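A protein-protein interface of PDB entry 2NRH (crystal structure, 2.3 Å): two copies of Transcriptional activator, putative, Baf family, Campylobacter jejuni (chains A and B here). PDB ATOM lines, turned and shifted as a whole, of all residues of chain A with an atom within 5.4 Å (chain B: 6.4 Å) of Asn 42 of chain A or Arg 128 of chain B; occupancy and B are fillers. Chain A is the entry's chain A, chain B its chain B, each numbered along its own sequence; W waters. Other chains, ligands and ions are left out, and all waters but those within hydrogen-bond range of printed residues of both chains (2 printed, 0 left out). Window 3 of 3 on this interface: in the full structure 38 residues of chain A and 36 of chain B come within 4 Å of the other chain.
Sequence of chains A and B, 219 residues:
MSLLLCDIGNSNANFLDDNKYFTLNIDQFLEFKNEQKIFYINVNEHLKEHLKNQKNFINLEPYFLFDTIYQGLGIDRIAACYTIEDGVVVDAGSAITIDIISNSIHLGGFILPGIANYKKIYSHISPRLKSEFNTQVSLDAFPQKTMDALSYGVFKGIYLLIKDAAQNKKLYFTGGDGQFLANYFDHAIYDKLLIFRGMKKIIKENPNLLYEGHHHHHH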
ATOM      1  N   ILE A   8      12.584  -5.734  34.063  1.00  0.00           N
ATOM      2  CA  ILE A   8      12.555  -6.306  32.739  1.00  0.00           C
ATOM      3  C   ILE A   8      12.654  -5.214  31.713  1.00  0.00           C
ATOM      4  O   ILE A   8      11.779  -4.389  31.630  1.00  0.00           O
ATOM      5  CB  ILE A   8      11.257  -7.081  32.496  1.00  0.00           C
ATOM      6  CG1 ILE A   8      11.067  -8.126  33.599  1.00  0.00           C
ATOM      7  CG2 ILE A   8      11.272  -7.696  31.108  1.00  0.00           C
ATOM      8  CD1 ILE A   8       9.711  -8.672  33.720  1.00  0.00           C
ATOM      9  N   GLY A   9      13.720  -5.230  30.915  1.00  0.00           N
ATOM     10  CA  GLY A   9      14.010  -4.164  29.964  1.00  0.00           C
ATOM     11  C   GLY A   9      13.851  -4.636  28.547  1.00  0.00           C
ATOM     12  O   GLY A   9      13.310  -5.714  28.287  1.00  0.00           O
ATOM     13  N   TYR A  40       7.794  -7.050  39.852  1.00  0.00           N
ATOM     14  CA  TYR A  40       8.428  -6.592  38.618  1.00  0.00           C
ATOM     15  C   TYR A  40       7.998  -5.238  38.112  1.00  0.00           C
ATOM     16  O   TYR A  40       6.903  -4.795  38.424  1.00  0.00           O
ATOM     17  CB  TYR A  40       8.274  -7.651  37.530  1.00  0.00           C
ATOM     18  CG  TYR A  40       6.937  -7.642  36.828  1.00  0.00           C
ATOM     19  CD1 TYR A  40       6.701  -6.781  35.737  1.00  0.00           C
ATOM     20  CD2 TYR A  40       5.912  -8.509  37.220  1.00  0.00           C
ATOM     21  CE1 TYR A  40       5.503  -6.780  35.083  1.00  0.00           C
ATOM     22  CE2 TYR A  40       4.694  -8.515  36.561  1.00  0.00           C
ATOM     23  CZ  TYR A  40       4.494  -7.648  35.501  1.00  0.00           C
ATOM     24  OH  TYR A  40       3.278  -7.628  34.854  1.00  0.00           O
ATOM     25  N   ILE A  41       8.897  -4.560  37.381  1.00  0.00           N
ATOM     26  CA  ILE A  41       8.544  -3.477  36.461  1.00  0.00           C
ATOM     27  C   ILE A  41       8.964  -3.923  35.063  1.00  0.00           C
ATOM     28  O   ILE A  41       9.890  -4.685  34.907  1.00  0.00           O
ATOM     29  CB  ILE A  41       9.183  -2.109  36.813  1.00  0.00           C
ATOM     30  CG1 ILE A  41      10.722  -2.177  36.794  1.00  0.00           C
ATOM     31  CG2 ILE A  41       8.704  -1.628  38.163  1.00  0.00           C
ATOM     32  CD1 ILE A  41      11.393  -0.867  36.879  1.00  0.00           C
ATOM     33  N   ASN A  42       8.244  -3.474  34.046  1.00  0.00           N
ATOM     34  CA  ASN A  42       8.528  -3.898  32.693  1.00  0.00           C
ATOM     35  C   ASN A  42       8.374  -2.748  31.716  1.00  0.00           C
ATOM     36  O   ASN A  42       7.365  -2.045  31.749  1.00  0.00           O
ATOM     37  CB  ASN A  42       7.632  -5.061  32.327  1.00  0.00           C
ATOM     38  CG  ASN A  42       7.676  -5.387  30.884  1.00  0.00           C
ATOM     39  OD1 ASN A  42       8.714  -5.781  30.344  1.00  0.00           O
ATOM     40  ND2 ASN A  42       6.519  -5.268  30.225  1.00  0.00           N
ATOM     41  N   VAL A  43       9.380  -2.517  30.874  1.00  0.00           N
ATOM     42  CA  VAL A  43       9.157  -1.633  29.722  1.00  0.00           C
ATOM     43  C   VAL A  43       9.087  -2.366  28.379  1.00  0.00           C
ATOM     44  O   VAL A  43       8.969  -1.726  27.331  1.00  0.00           O
ATOM     45  CB  VAL A  43      10.206  -0.529  29.627  1.00  0.00           C
ATOM     46  CG1 VAL A  43      10.084   0.425  30.818  1.00  0.00           C
ATOM     47  CG2 VAL A  43      11.605  -1.153  29.483  1.00  0.00           C
ATOM     48  N   ASN A  44       9.201  -3.695  28.407  1.00  0.00           N
ATOM     49  CA  ASN A  44       9.227  -4.490  27.145  1.00  0.00           C
ATOM     50  C   ASN A  44       7.781  -4.727  26.585  1.00  0.00           C
ATOM     51  O   ASN A  44       7.078  -5.664  27.017  1.00  0.00           O
ATOM     52  CB  ASN A  44      10.050  -5.790  27.357  1.00  0.00           C
ATOM     53  CG  ASN A  44      10.425  -6.530  26.054  1.00  0.00           C
ATOM     54  OD1 ASN A  44       9.577  -6.806  25.220  1.00  0.00           O
ATOM     55  ND2 ASN A  44      11.687  -6.937  25.938  1.00  0.00           N
ATOM     56  N   GLU A  45       7.352  -3.875  25.641  1.00  0.00           N
ATOM     57  CA  GLU A  45       6.084  -4.090  24.936  1.00  0.00           C
ATOM     58  C   GLU A  45       5.763  -5.515  24.599  1.00  0.00           C
ATOM     59  O   GLU A  45       4.666  -5.975  24.916  1.00  0.00           O
ATOM     60  CB  GLU A  45       5.927  -3.259  23.649  1.00  0.00           C
ATOM     61  CG  GLU A  45       5.189  -1.912  23.826  1.00  0.00           C
ATOM     62  CD  GLU A  45       3.867  -1.988  24.646  1.00  0.00           C
ATOM     63  OE1 GLU A  45       2.960  -2.836  24.381  1.00  0.00           O
ATOM     64  OE2 GLU A  45       3.752  -1.160  25.569  1.00  0.00           O
ATOM     65  N   LEU A  47       6.611  -8.135  25.689  1.00  0.00           N
ATOM     66  CA  LEU A  47       6.507  -8.972  26.883  1.00  0.00           C
ATOM     67  C   LEU A  47       5.247  -8.714  27.755  1.00  0.00           C
ATOM     68  O   LEU A  47       5.047  -9.411  28.756  1.00  0.00           O
ATOM     69  CB  LEU A  47       7.785  -8.845  27.730  1.00  0.00           C
ATOM     70  CG  LEU A  47       9.056  -9.568  27.258  1.00  0.00           C
ATOM     71  CD1 LEU A  47      10.077  -9.550  28.359  1.00  0.00           C
ATOM     72  CD2 LEU A  47       8.808 -11.007  26.892  1.00  0.00           C
ATOM     73  N   LYS A  48       4.412  -7.734  27.404  1.00  0.00           N
ATOM     74  CA  LYS A  48       3.217  -7.473  28.216  1.00  0.00           C
ATOM     75  C   LYS A  48       2.352  -8.739  28.444  1.00  0.00           C
ATOM     76  O   LYS A  48       2.096  -9.123  29.595  1.00  0.00           O
ATOM     77  CB  LYS A  48       2.359  -6.360  27.613  1.00  0.00           C
ATOM     78  CG  LYS A  48       2.660  -4.972  28.120  1.00  0.00           C
ATOM     79  CD  LYS A  48       1.869  -3.929  27.344  1.00  0.00           C
ATOM     80  CE  LYS A  48       0.575  -3.613  28.036  1.00  0.00           C
ATOM     81  NZ  LYS A  48       0.840  -3.292  29.475  1.00  0.00           N
ATOM     82  N   LEU A  51       3.628 -11.749  30.645  1.00  0.00           N
ATOM     83  CA  LEU A  51       3.750 -11.421  32.048  1.00  0.00           C
ATOM     84  C   LEU A  51       2.407 -11.537  32.749  1.00  0.00           C
ATOM     85  O   LEU A  51       2.346 -12.027  33.882  1.00  0.00           O
ATOM     86  CB  LEU A  51       4.345 -10.025  32.234  1.00  0.00           C
ATOM     87  CG  LEU A  51       5.856  -9.885  32.070  1.00  0.00           C
ATOM     88  CD1 LEU A  51       6.247  -8.503  31.508  1.00  0.00           C
ATOM     89  CD2 LEU A  51       6.526 -10.188  33.410  1.00  0.00           C
ATOM     90  N   ASN A  59       2.946  -7.065  39.194  1.00  0.00           N
ATOM     91  CA  ASN A  59       3.361  -5.766  38.640  1.00  0.00           C
ATOM     92  C   ASN A  59       3.385  -4.711  39.731  1.00  0.00           C
ATOM     93  O   ASN A  59       2.460  -4.654  40.514  1.00  0.00           O
ATOM     94  CB  ASN A  59       2.457  -5.338  37.478  1.00  0.00           C
ATOM     95  CG  ASN A  59       3.127  -4.316  36.532  1.00  0.00           C
ATOM     96  OD1 ASN A  59       3.984  -3.544  36.928  1.00  0.00           O
ATOM     97  ND2 ASN A  59       2.693  -4.309  35.278  1.00  0.00           N
ATOM     98  N   GLU A  61       4.290  -1.355  38.925  1.00  0.00           N
ATOM     99  CA  GLU A  61       4.060  -0.045  38.313  1.00  0.00           C
ATOM    100  C   GLU A  61       2.912   0.831  38.897  1.00  0.00           C
ATOM    101  O   GLU A  61       3.105   2.046  39.123  1.00  0.00           O
ATOM    102  CB  GLU A  61       3.865  -0.209  36.800  1.00  0.00           C
ATOM    103  CG  GLU A  61       3.627   1.100  36.081  1.00  0.00           C
ATOM    104  CD  GLU A  61       3.902   1.002  34.605  1.00  0.00           C
ATOM    105  OE1 GLU A  61       4.248  -0.124  34.160  1.00  0.00           O
ATOM    106  OE2 GLU A  61       3.799   2.052  33.897  1.00  0.00           O
ATOM    107  N   GLY A  74       8.381   6.504  31.433  1.00  0.00           N
ATOM    108  CA  GLY A  74       8.540   5.084  31.619  1.00  0.00           C
ATOM    109  C   GLY A  74       8.857   4.669  33.037  1.00  0.00           C
ATOM    110  O   GLY A  74       9.430   5.430  33.801  1.00  0.00           O
ATOM    111  N   ILE A  75       8.496   3.440  33.380  1.00  0.00           N
ATOM    112  CA  ILE A  75       8.526   2.990  34.776  1.00  0.00           C
ATOM    113  C   ILE A  75       9.967   2.683  35.213  1.00  0.00           C
ATOM    114  O   ILE A  75      10.306   2.764  36.395  1.00  0.00           O
ATOM    115  CB  ILE A  75       7.504   1.805  35.048  1.00  0.00           C
ATOM    116  CG1 ILE A  75       7.323   1.521  36.558  1.00  0.00           C
ATOM    117  CG2 ILE A  75       7.848   0.508  34.288  1.00  0.00           C
ATOM    118  CD1 ILE A  75       7.052   2.793  37.349  1.00  0.00           C
ATOM    119  N   TYR B 122      15.617   3.874  17.328  1.00  0.00           N
ATOM    120  CA  TYR B 122      14.635   4.063  18.418  1.00  0.00           C
ATOM    121  C   TYR B 122      13.481   3.051  18.284  1.00  0.00           C
ATOM    122  O   TYR B 122      13.189   2.267  19.224  1.00  0.00           O
ATOM    123  CB  TYR B 122      14.106   5.492  18.440  1.00  0.00           C
ATOM    124  CG  TYR B 122      15.053   6.483  19.079  1.00  0.00           C
ATOM    125  CD1 TYR B 122      15.731   6.183  20.294  1.00  0.00           C
ATOM    126  CD2 TYR B 122      15.259   7.736  18.512  1.00  0.00           C
ATOM    127  CE1 TYR B 122      16.585   7.127  20.916  1.00  0.00           C
ATOM    128  CE2 TYR B 122      16.100   8.658  19.113  1.00  0.00           C
ATOM    129  CZ  TYR B 122      16.782   8.347  20.308  1.00  0.00           C
ATOM    130  OH  TYR B 122      17.600   9.341  20.887  1.00  0.00           O
ATOM    131  N   SER B 126      12.238   0.080  20.824  1.00  0.00           N
ATOM    132  CA  SER B 126      10.891  -0.075  21.366  1.00  0.00           C
ATOM    133  C   SER B 126       9.860   0.709  20.546  1.00  0.00           C
ATOM    134  O   SER B 126      10.160   1.802  20.029  1.00  0.00           O
ATOM    135  CB  SER B 126      10.833   0.327  22.855  1.00  0.00           C
ATOM    136  OG  SER B 126       9.602  -0.033  23.469  1.00  0.00           O
ATOM    137  N   PRO B 127       8.647   0.123  20.403  1.00  0.00           N
ATOM    138  CA  PRO B 127       7.499   0.897  19.886  1.00  0.00           C
ATOM    139  C   PRO B 127       7.143   2.114  20.756  1.00  0.00           C
ATOM    140  O   PRO B 127       6.581   3.087  20.242  1.00  0.00           O
ATOM    141  CB  PRO B 127       6.350  -0.119  19.824  1.00  0.00           C
ATOM    142  CG  PRO B 127       6.842  -1.394  20.528  1.00  0.00           C
ATOM    143  CD  PRO B 127       8.333  -1.306  20.666  1.00  0.00           C
ATOM    144  N   ARG B 128       7.503   2.095  22.038  1.00  0.00           N
ATOM    145  CA  ARG B 128       7.353   3.301  22.846  1.00  0.00           C
ATOM    146  C   ARG B 128       8.256   4.418  22.419  1.00  0.00           C
ATOM    147  O   ARG B 128       7.993   5.569  22.746  1.00  0.00           O
ATOM    148  CB  ARG B 128       7.594   3.038  24.315  1.00  0.00           C
ATOM    149  CG  ARG B 128       6.460   2.295  24.998  1.00  0.00           C
ATOM    150  CD  ARG B 128       6.569   2.578  26.463  1.00  0.00           C
ATOM    151  NE  ARG B 128       6.148   1.493  27.352  1.00  0.00           N
ATOM    152  CZ  ARG B 128       6.486   1.445  28.640  1.00  0.00           C
ATOM    153  NH1 ARG B 128       7.253   2.415  29.154  1.00  0.00           N
ATOM    154  NH2 ARG B 128       6.056   0.443  29.410  1.00  0.00           N
ATOM    155  N   LEU B 129       9.322   4.088  21.683  1.00  0.00           N
ATOM    156  CA  LEU B 129      10.229   5.099  21.128  1.00  0.00           C
ATOM    157  C   LEU B 129      10.058   5.253  19.604  1.00  0.00           C
ATOM    158  O   LEU B 129      10.746   6.080  18.982  1.00  0.00           O
ATOM    159  CB  LEU B 129      11.677   4.788  21.518  1.00  0.00           C
ATOM    160  CG  LEU B 129      11.870   4.277  22.971  1.00  0.00           C
ATOM    161  CD1 LEU B 129      13.324   3.858  23.185  1.00  0.00           C
ATOM    162  CD2 LEU B 129      11.441   5.324  24.053  1.00  0.00           C
ATOM    163  N   THR B 146       7.834  12.109  25.455  1.00  0.00           N
ATOM    164  CA  THR B 146       8.727  11.203  24.745  1.00  0.00           C
ATOM    165  C   THR B 146       9.177  11.610  23.324  1.00  0.00           C
ATOM    166  O   THR B 146      10.349  11.404  22.979  1.00  0.00           O
ATOM    167  CB  THR B 146       8.251   9.729  24.805  1.00  0.00           C
ATOM    168  OG1 THR B 146       8.343   9.274  26.158  1.00  0.00           O
ATOM    169  CG2 THR B 146       9.140   8.844  23.975  1.00  0.00           C
ATOM    170  N   LEU B 150      13.310  12.163  22.628  1.00  0.00           N
ATOM    171  CA  LEU B 150      14.023  11.705  21.442  1.00  0.00           C
ATOM    172  C   LEU B 150      14.626  12.825  20.599  1.00  0.00           C
ATOM    173  O   LEU B 150      15.820  12.774  20.196  1.00  0.00           O
ATOM    174  CB  LEU B 150      13.087  10.849  20.579  1.00  0.00           C
ATOM    175  CG  LEU B 150      12.484   9.608  21.297  1.00  0.00           C
ATOM    176  CD1 LEU B 150      11.352   8.973  20.481  1.00  0.00           C
ATOM    177  CD2 LEU B 150      13.487   8.520  21.773  1.00  0.00           C
HETATM  178  O   HOH W   1       6.047   2.441  31.766  1.00  0.00           O
HETATM  179  O   HOH W   2      10.125   0.363  26.125  1.00  0.00           O
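The backbone NH (N) of Arg 128 of chain B lies close to the side-chain hydroxyl (OG) of Ser 126 of chain B, at 3.3 Å. The backbone carbonyl oxygen (O) of Ile 8 of chain A is in hydrogen-bond range of the backbone NH (N) of Val 43 of chain A (3.1 Å). The side-chain amide oxygen of Asn 42 of chain A sits at hydrogen-bond distance from the backbone NH of Asn 44 of chain A, 2.9 Å away.
Printed residues of chain A that touch a printed residue of chain B: Asn 42, Val 43, Glu 45 and Gly 74. Hydrophobic or aromatic side chains of chain A that line the printed part of chain B: Val 43. Printed residues of chain B that touch a printed residue of chain A: Pro 127 and Arg 128. Along chain B the printed residues that touch a printed residue of chain A span positions 127 to 128. Among the printed residues, Asp or Glu carboxylates within 4 Å of a Lys or Arg side-chain nitrogen of the other chain: Glu 45 of chain A with Arg 128 of chain B.
Among the printed residues, merely in contact across the chains: Asn 42 of chain A with Arg 128 of chain B, Val 43 of chain A with Arg 128 of chain B, Glu 45 of chain A with Pro 127 of chain B and Gly 74 of chain A with Arg 128 of chain B.
No position is printed for both chains.
Of chain B, only Arg 128 comes within 4 Å of Asn 42 of chain A. Of the printed residues of chain B, Val 43 of chain A touches Arg 128 (3.7 Å). Printed residues of chain B within 4 Å of Glu 45 of chain A: Pro 127 and Arg 128. Of the printed residues of chain B, Gly 74 of chain A touches Arg 128. Of the printed residues of chain A, Pro 127 of chain B touches Glu 45 (3.7 Å). Printed residues of chain A within 4 Å of Arg 128 of chain B: Asn 42 (3.7 Å), Val 43 (3.7 Å), Glu 45 (3.99 Å) and Gly 74 (3.9 Å). The nearest printed residue of chain B that does not touch Asn 42 of chain A is Ser 126 of chain B (8.8 Å). The nearest printed residue of chain A that does not touch Arg 128 of chain B is Ile 75 of chain A (4.5 Å). The nearest printed residue of chain B that does not touch Glu 45 of chain A is Ser 126 of chain B (4.8 Å).
Water W2 bridges the backbone carbonyl oxygen of Val 43 of chain A (2.7 Å) and the side-chain hydroxyl of Ser 126 of chain B (2.7 Å). Water W1 lies within hydrogen-bond range of NH1 of Arg 128 of chain B, N of Ile 75 of chain A and OE2 of Glu 61 of chain A.
OE2 of Glu 45 of chain A is in salt-bridge range of NE of Arg 128 of chain B, 3.99 Å away.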
